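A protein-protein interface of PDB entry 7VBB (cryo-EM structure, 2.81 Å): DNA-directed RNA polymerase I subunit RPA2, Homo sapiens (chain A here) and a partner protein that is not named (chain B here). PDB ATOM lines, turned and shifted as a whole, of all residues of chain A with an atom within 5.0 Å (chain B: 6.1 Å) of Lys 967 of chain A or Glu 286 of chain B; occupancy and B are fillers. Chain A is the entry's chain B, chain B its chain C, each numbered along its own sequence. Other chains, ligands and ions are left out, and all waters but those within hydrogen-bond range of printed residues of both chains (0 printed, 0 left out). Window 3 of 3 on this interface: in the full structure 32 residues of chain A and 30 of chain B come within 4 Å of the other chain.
Lys 967 of chain A touches one residue of chain B.
Glu 286 of chain B touches just these residues of chain A: Lys 967 (3.5 Å), Tyr 971 (3.7 Å), Asn 972 (2.9 Å) and Phe 973 (2.6 Å).
Of the printed residues of chain B, Gly 970 of chain A touches Ser 284.
Of the printed residues of chain A, Ser 284 of chain B touches Gly 970 (3.6 Å), Tyr 971 (3.9 Å) and Asn 972 (2.9 Å).
Printed residues of chain B within 4 Å of Asn 972 of chain A: Ser 284, Arg 285 and Glu 286.
Of the printed residues of chain B, Phe 973 of chain A touches Glu 286 and Arg 289.
Of the printed residues of chain A, Arg 285 of chain B touches Asn 972 (3.97 Å).
Met 965 of chain A touches none of the printed residues of chain B.
Glu 964 of chain A touches none of the printed residues of chain B.
The nearest residue of chain B that does not touch Lys 967 of chain A is Arg 289 of chain B (4.3 Å).
The nearest printed residue of chain B that does not touch Asn 972 of chain A is Arg 289 of chain B (6.5 Å).
OE1 of Glu 286 of chain B touches CG of Lys 967 of chain A (3.5 Å).
Gly 970 of chain A touches Ser 284 of chain B (O to CB, 3.6 Å).
Tyr 971 of chain A touches Ser 284 of chain B (O to CB, 3.9 Å).
OE2 of Glu 286 of chain B touches O of Tyr 971 of chain A, at 3.7 Å.
Asn 972 of chain A touches Ser 284 of chain B (CB to O, 2.9 Å).
ND2 of Asn 972 of chain A touches NH2 of Arg 285 of chain B, at 3.97 Å.
CA of Asn 972 of chain A touches OE2 of Glu 286 of chain B, at 2.9 Å.
CD of Arg 289 of chain B touches CB of Phe 973 of chain A, at 3.6 Å.
Of the 11 printed residues of chain A, 5 touch a printed residue of chain B.
Along chain A the printed residues that touch a printed residue of chain B span positions 967 to 973.
Along chain B the printed residues that touch a printed residue of chain A span positions 284 to 289.
OE2 of Glu 286 of chain B is in hydrogen-bond range of N of Phe 973 of chain A (2.6 Å).
The backbone NH (N) of Tyr 971 of chain A sits at hydrogen-bond distance from the backbone carbonyl oxygen (O) of Leu 966 of chain A (3.4 Å).
The side-chain carboxylate (OE1) of Glu 286 of chain B lies within salt-bridge range of the guanidinium group (NH1) of Arg 289 of chain B (3.8 Å).
The side-chain carboxylate (OE1) of Glu 964 of chain A lies within salt-bridge range of the side-chain amino group (NZ) of Lys 967 of chain A (3.3 Å).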
ATOM      1  N   GLY A 963      10.416  -0.020  28.301  1.00  0.00           N
ATOM      2  CA  GLY A 963      11.351   1.012  27.906  1.00  0.00           C
ATOM      3  C   GLY A 963      12.400   1.260  28.968  1.00  0.00           C
ATOM      4  O   GLY A 963      13.555   1.538  28.653  1.00  0.00           O
ATOM      5  N   GLU A 964      12.014   1.163  30.241  1.00  0.00           N
ATOM      6  CA  GLU A 964      13.017   1.208  31.297  1.00  0.00           C
ATOM      7  C   GLU A 964      13.963   0.022  31.204  1.00  0.00           C
ATOM      8  O   GLU A 964      15.181   0.187  31.346  1.00  0.00           O
ATOM      9  CB  GLU A 964      12.340   1.248  32.663  1.00  0.00           C
ATOM     10  CG  GLU A 964      11.708   2.586  32.998  1.00  0.00           C
ATOM     11  CD  GLU A 964      12.735   3.657  33.313  1.00  0.00           C
ATOM     12  OE1 GLU A 964      12.857   4.616  32.525  1.00  0.00           O
ATOM     13  OE2 GLU A 964      13.419   3.543  34.350  1.00  0.00           O
ATOM     14  N   MET A 965      13.427  -1.172  30.947  1.00  0.00           N
ATOM     15  CA  MET A 965      14.284  -2.336  30.732  1.00  0.00           C
ATOM     16  C   MET A 965      15.281  -2.089  29.606  1.00  0.00           C
ATOM     17  O   MET A 965      16.473  -2.378  29.746  1.00  0.00           O
ATOM     18  CB  MET A 965      13.435  -3.569  30.428  1.00  0.00           C
ATOM     19  CG  MET A 965      12.623  -4.078  31.597  1.00  0.00           C
ATOM     20  SD  MET A 965      13.666  -4.795  32.873  1.00  0.00           S
ATOM     21  CE  MET A 965      12.433  -5.354  34.042  1.00  0.00           C
ATOM     22  N   LEU A 966      14.808  -1.560  28.475  1.00  0.00           N
ATOM     23  CA  LEU A 966      15.698  -1.301  27.345  1.00  0.00           C
ATOM     24  C   LEU A 966      16.740  -0.242  27.684  1.00  0.00           C
ATOM     25  O   LEU A 966      17.937  -0.448  27.458  1.00  0.00           O
ATOM     26  CB  LEU A 966      14.889  -0.874  26.125  1.00  0.00           C
ATOM     27  CG  LEU A 966      14.213  -1.994  25.343  1.00  0.00           C
ATOM     28  CD1 LEU A 966      13.279  -1.416  24.303  1.00  0.00           C
ATOM     29  CD2 LEU A 966      15.257  -2.875  24.700  1.00  0.00           C
ATOM     30  N   LYS A 967      16.308   0.901  28.213  1.00  0.00           N
ATOM     31  CA  LYS A 967      17.236   1.956  28.591  1.00  0.00           C
ATOM     32  C   LYS A 967      18.249   1.491  29.624  1.00  0.00           C
ATOM     33  O   LYS A 967      19.320   2.095  29.741  1.00  0.00           O
ATOM     34  CB  LYS A 967      16.458   3.160  29.118  1.00  0.00           C
ATOM     35  CG  LYS A 967      17.311   4.359  29.456  1.00  0.00           C
ATOM     36  CD  LYS A 967      17.421   4.539  30.955  1.00  0.00           C
ATOM     37  CE  LYS A 967      16.101   4.993  31.546  1.00  0.00           C
ATOM     38  NZ  LYS A 967      16.139   5.018  33.034  1.00  0.00           N
ATOM     39  N   ALA A 968      17.939   0.441  30.380  1.00  0.00           N
ATOM     40  CA  ALA A 968      18.901  -0.138  31.304  1.00  0.00           C
ATOM     41  C   ALA A 968      19.919  -1.034  30.613  1.00  0.00           C
ATOM     42  O   ALA A 968      20.850  -1.510  31.270  1.00  0.00           O
ATOM     43  CB  ALA A 968      18.178  -0.929  32.395  1.00  0.00           C
ATOM     44  N   ALA A 969      19.768  -1.274  29.311  1.00  0.00           N
ATOM     45  CA  ALA A 969      20.705  -2.093  28.553  1.00  0.00           C
ATOM     46  C   ALA A 969      21.532  -1.275  27.575  1.00  0.00           C
ATOM     47  O   ALA A 969      22.302  -1.850  26.800  1.00  0.00           O
ATOM     48  CB  ALA A 969      19.963  -3.199  27.797  1.00  0.00           C
ATOM     49  N   GLY A 970      21.396   0.048  27.585  1.00  0.00           N
ATOM     50  CA  GLY A 970      22.102   0.897  26.656  1.00  0.00           C
ATOM     51  C   GLY A 970      21.342   1.224  25.392  1.00  0.00           C
ATOM     52  O   GLY A 970      21.818   2.043  24.598  1.00  0.00           O
ATOM     53  N   TYR A 971      20.188   0.611  25.174  1.00  0.00           N
ATOM     54  CA  TYR A 971      19.332   0.959  24.054  1.00  0.00           C
ATOM     55  C   TYR A 971      18.462   2.139  24.476  1.00  0.00           C
ATOM     56  O   TYR A 971      18.652   2.715  25.548  1.00  0.00           O
ATOM     57  CB  TYR A 971      18.542  -0.266  23.607  1.00  0.00           C
ATOM     58  CG  TYR A 971      19.394  -1.256  22.852  1.00  0.00           C
ATOM     59  CD1 TYR A 971      20.371  -1.995  23.499  1.00  0.00           C
ATOM     60  CD2 TYR A 971      19.238  -1.435  21.488  1.00  0.00           C
ATOM     61  CE1 TYR A 971      21.159  -2.888  22.812  1.00  0.00           C
ATOM     62  CE2 TYR A 971      20.022  -2.330  20.792  1.00  0.00           C
ATOM     63  CZ  TYR A 971      20.980  -3.053  21.457  1.00  0.00           C
ATOM     64  OH  TYR A 971      21.761  -3.946  20.764  1.00  0.00           O
ATOM     65  N   ASN A 972      17.503   2.531  23.646  1.00  0.00           N
ATOM     66  CA  ASN A 972      16.722   3.725  23.925  1.00  0.00           C
ATOM     67  C   ASN A 972      15.322   3.353  24.392  1.00  0.00           C
ATOM     68  O   ASN A 972      14.800   2.289  24.050  1.00  0.00           O
ATOM     69  CB  ASN A 972      16.645   4.644  22.704  1.00  0.00           C
ATOM     70  CG  ASN A 972      15.643   4.180  21.692  1.00  0.00           C
ATOM     71  OD1 ASN A 972      15.470   2.982  21.484  1.00  0.00           O
ATOM     72  ND2 ASN A 972      14.969   5.125  21.054  1.00  0.00           N
ATOM     73  N   PHE A 973      14.732   4.250  25.182  1.00  0.00           N
ATOM     74  CA  PHE A 973      13.429   4.002  25.781  1.00  0.00           C
ATOM     75  C   PHE A 973      12.430   3.494  24.751  1.00  0.00           C
ATOM     76  O   PHE A 973      11.870   2.404  24.898  1.00  0.00           O
ATOM     77  CB  PHE A 973      12.917   5.291  26.422  1.00  0.00           C
ATOM     78  CG  PHE A 973      11.706   5.105  27.284  1.00  0.00           C
ATOM     79  CD1 PHE A 973      11.836   4.783  28.621  1.00  0.00           C
ATOM     80  CD2 PHE A 973      10.437   5.228  26.753  1.00  0.00           C
ATOM     81  CE1 PHE A 973      10.727   4.620  29.413  1.00  0.00           C
ATOM     82  CE2 PHE A 973       9.324   5.056  27.542  1.00  0.00           C
ATOM     83  CZ  PHE A 973       9.471   4.751  28.874  1.00  0.00           C
ATOM     84  N   ARG B 255      25.116   9.815  32.612  1.00  0.00           N
ATOM     85  CA  ARG B 255      24.298   8.610  32.618  1.00  0.00           C
ATOM     86  C   ARG B 255      23.407   8.497  31.389  1.00  0.00           C
ATOM     87  O   ARG B 255      22.925   7.400  31.085  1.00  0.00           O
ATOM     88  CB  ARG B 255      23.438   8.556  33.883  1.00  0.00           C
ATOM     89  CG  ARG B 255      24.143   7.934  35.074  1.00  0.00           C
ATOM     90  CD  ARG B 255      23.219   7.835  36.271  1.00  0.00           C
ATOM     91  NE  ARG B 255      22.979   9.136  36.886  1.00  0.00           N
ATOM     92  CZ  ARG B 255      21.848   9.473  37.495  1.00  0.00           C
ATOM     93  NH1 ARG B 255      20.848   8.604  37.569  1.00  0.00           N
ATOM     94  NH2 ARG B 255      21.714  10.679  38.028  1.00  0.00           N
ATOM     95  N   CYS B 256      23.181   9.594  30.675  1.00  0.00           N
ATOM     96  CA  CYS B 256      22.377   9.576  29.459  1.00  0.00           C
ATOM     97  C   CYS B 256      23.168   9.134  28.236  1.00  0.00           C
ATOM     98  O   CYS B 256      22.630   9.150  27.124  1.00  0.00           O
ATOM     99  CB  CYS B 256      21.765  10.957  29.215  1.00  0.00           C
ATOM    100  SG  CYS B 256      20.752  11.575  30.577  1.00  0.00           S
ATOM    101  N   PHE B 257      24.378   8.631  28.452  1.00  0.00           N
ATOM    102  CA  PHE B 257      25.258   8.233  27.328  1.00  0.00           C
ATOM    103  C   PHE B 257      25.858   6.877  27.649  1.00  0.00           C
ATOM    104  O   PHE B 257      25.719   6.445  28.782  1.00  0.00           O
ATOM    105  CB  PHE B 257      26.380   9.258  27.175  1.00  0.00           C
ATOM    106  CG  PHE B 257      26.045  10.440  26.305  1.00  0.00           C
ATOM    107  CD1 PHE B 257      25.934  10.298  24.934  1.00  0.00           C
ATOM    108  CD2 PHE B 257      25.838  11.692  26.855  1.00  0.00           C
ATOM    109  CE1 PHE B 257      25.620  11.379  24.130  1.00  0.00           C
ATOM    110  CE2 PHE B 257      25.530  12.774  26.049  1.00  0.00           C
ATOM    111  CZ  PHE B 257      25.419  12.616  24.690  1.00  0.00           C
ATOM    112  N   SER B 284      21.456   6.258  21.503  1.00  0.00           N
ATOM    113  CA  SER B 284      20.311   5.833  22.325  1.00  0.00           C
ATOM    114  C   SER B 284      19.471   7.078  22.537  1.00  0.00           C
ATOM    115  O   SER B 284      18.332   6.953  22.940  1.00  0.00           O
ATOM    116  CB  SER B 284      20.807   5.316  23.600  1.00  0.00           C
ATOM    117  OG  SER B 284      21.894   6.085  24.081  1.00  0.00           O
ATOM    118  N   ARG B 285      20.038   8.247  22.287  1.00  0.00           N
ATOM    119  CA  ARG B 285      19.254   9.476  22.325  1.00  0.00           C
ATOM    120  C   ARG B 285      18.476   9.580  23.631  1.00  0.00           C
ATOM    121  O   ARG B 285      17.310   9.974  23.655  1.00  0.00           O
ATOM    122  CB  ARG B 285      18.308   9.571  21.127  1.00  0.00           C
ATOM    123  CG  ARG B 285      18.984   9.921  19.813  1.00  0.00           C
ATOM    124  CD  ARG B 285      19.432   8.666  19.093  1.00  0.00           C
ATOM    125  NE  ARG B 285      18.278   7.878  18.666  1.00  0.00           N
ATOM    126  CZ  ARG B 285      18.335   6.608  18.280  1.00  0.00           C
ATOM    127  NH1 ARG B 285      19.493   5.965  18.272  1.00  0.00           N
ATOM    128  NH2 ARG B 285      17.230   5.980  17.910  1.00  0.00           N
ATOM    129  N   GLU B 286      19.127   9.219  24.733  1.00  0.00           N
ATOM    130  CA  GLU B 286      18.494   9.308  26.040  1.00  0.00           C
ATOM    131  C   GLU B 286      18.642  10.682  26.680  1.00  0.00           C
ATOM    132  O   GLU B 286      17.966  10.957  27.675  1.00  0.00           O
ATOM    133  CB  GLU B 286      19.058   8.244  26.984  1.00  0.00           C
ATOM    134  CG  GLU B 286      18.676   6.832  26.597  1.00  0.00           C
ATOM    135  CD  GLU B 286      17.186   6.596  26.699  1.00  0.00           C
ATOM    136  OE1 GLU B 286      16.545   7.219  27.569  1.00  0.00           O
ATOM    137  OE2 GLU B 286      16.653   5.793  25.906  1.00  0.00           O
ATOM    138  N   ILE B 287      19.508  11.539  26.140  1.00  0.00           N
ATOM    139  CA  ILE B 287      19.521  12.930  26.577  1.00  0.00           C
ATOM    140  C   ILE B 287      18.228  13.619  26.172  1.00  0.00           C
ATOM    141  O   ILE B 287      17.700  14.453  26.918  1.00  0.00           O
ATOM    142  CB  ILE B 287      20.747  13.661  26.005  1.00  0.00           C
ATOM    143  CG1 ILE B 287      20.986  13.232  24.560  1.00  0.00           C
ATOM    144  CG2 ILE B 287      21.970  13.392  26.853  1.00  0.00           C
ATOM    145  CD1 ILE B 287      21.964  14.104  23.825  1.00  0.00           C
ATOM    146  N   PHE B 288      17.693  13.280  25.002  1.00  0.00           N
ATOM    147  CA  PHE B 288      16.477  13.897  24.485  1.00  0.00           C
ATOM    148  C   PHE B 288      15.264  13.657  25.369  1.00  0.00           C
ATOM    149  O   PHE B 288      14.219  14.272  25.131  1.00  0.00           O
ATOM    150  CB  PHE B 288      16.203  13.384  23.074  1.00  0.00           C
ATOM    151  CG  PHE B 288      17.265  13.756  22.086  1.00  0.00           C
ATOM    152  CD1 PHE B 288      18.141  14.791  22.353  1.00  0.00           C
ATOM    153  CD2 PHE B 288      17.400  13.064  20.899  1.00  0.00           C
ATOM    154  CE1 PHE B 288      19.124  15.138  21.450  1.00  0.00           C
ATOM    155  CE2 PHE B 288      18.382  13.407  19.991  1.00  0.00           C
ATOM    156  CZ  PHE B 288      19.244  14.446  20.268  1.00  0.00           C
ATOM    157  N   ARG B 289      15.362  12.784  26.368  1.00  0.00           N
ATOM    158  CA  ARG B 289      14.301  12.595  27.344  1.00  0.00           C
ATOM    159  C   ARG B 289      14.507  13.441  28.588  1.00  0.00           C
ATOM    160  O   ARG B 289      13.685  13.381  29.510  1.00  0.00           O
ATOM    161  CB  ARG B 289      14.189  11.121  27.737  1.00  0.00           C
ATOM    162  CG  ARG B 289      13.636  10.216  26.657  1.00  0.00           C
ATOM    163  CD  ARG B 289      13.372   8.825  27.206  1.00  0.00           C
ATOM    164  NE  ARG B 289      12.306   8.828  28.202  1.00  0.00           N
ATOM    165  CZ  ARG B 289      12.476   8.502  29.478  1.00  0.00           C
ATOM    166  NH1 ARG B 289      13.672   8.146  29.922  1.00  0.00           N
ATOM    167  NH2 ARG B 289      11.447   8.533  30.314  1.00  0.00           N
ATOM    168  N   ASN B 290      15.581  14.229  28.641  1.00  0.00           N
ATOM    169  CA  ASN B 290      15.935  14.953  29.852  1.00  0.00           C
ATOM    170  C   ASN B 290      15.233  16.297  29.982  1.00  0.00           C
ATOM    171  O   ASN B 290      15.007  16.751  31.109  1.00  0.00           O
ATOM    172  CB  ASN B 290      17.451  15.169  29.917  1.00  0.00           C
ATOM    173  CG  ASN B 290      17.918  15.601  31.291  1.00  0.00           C
ATOM    174  OD1 ASN B 290      17.119  15.724  32.220  1.00  0.00           O
ATOM    175  ND2 ASN B 290      19.212  15.842  31.428  1.00  0.00           N
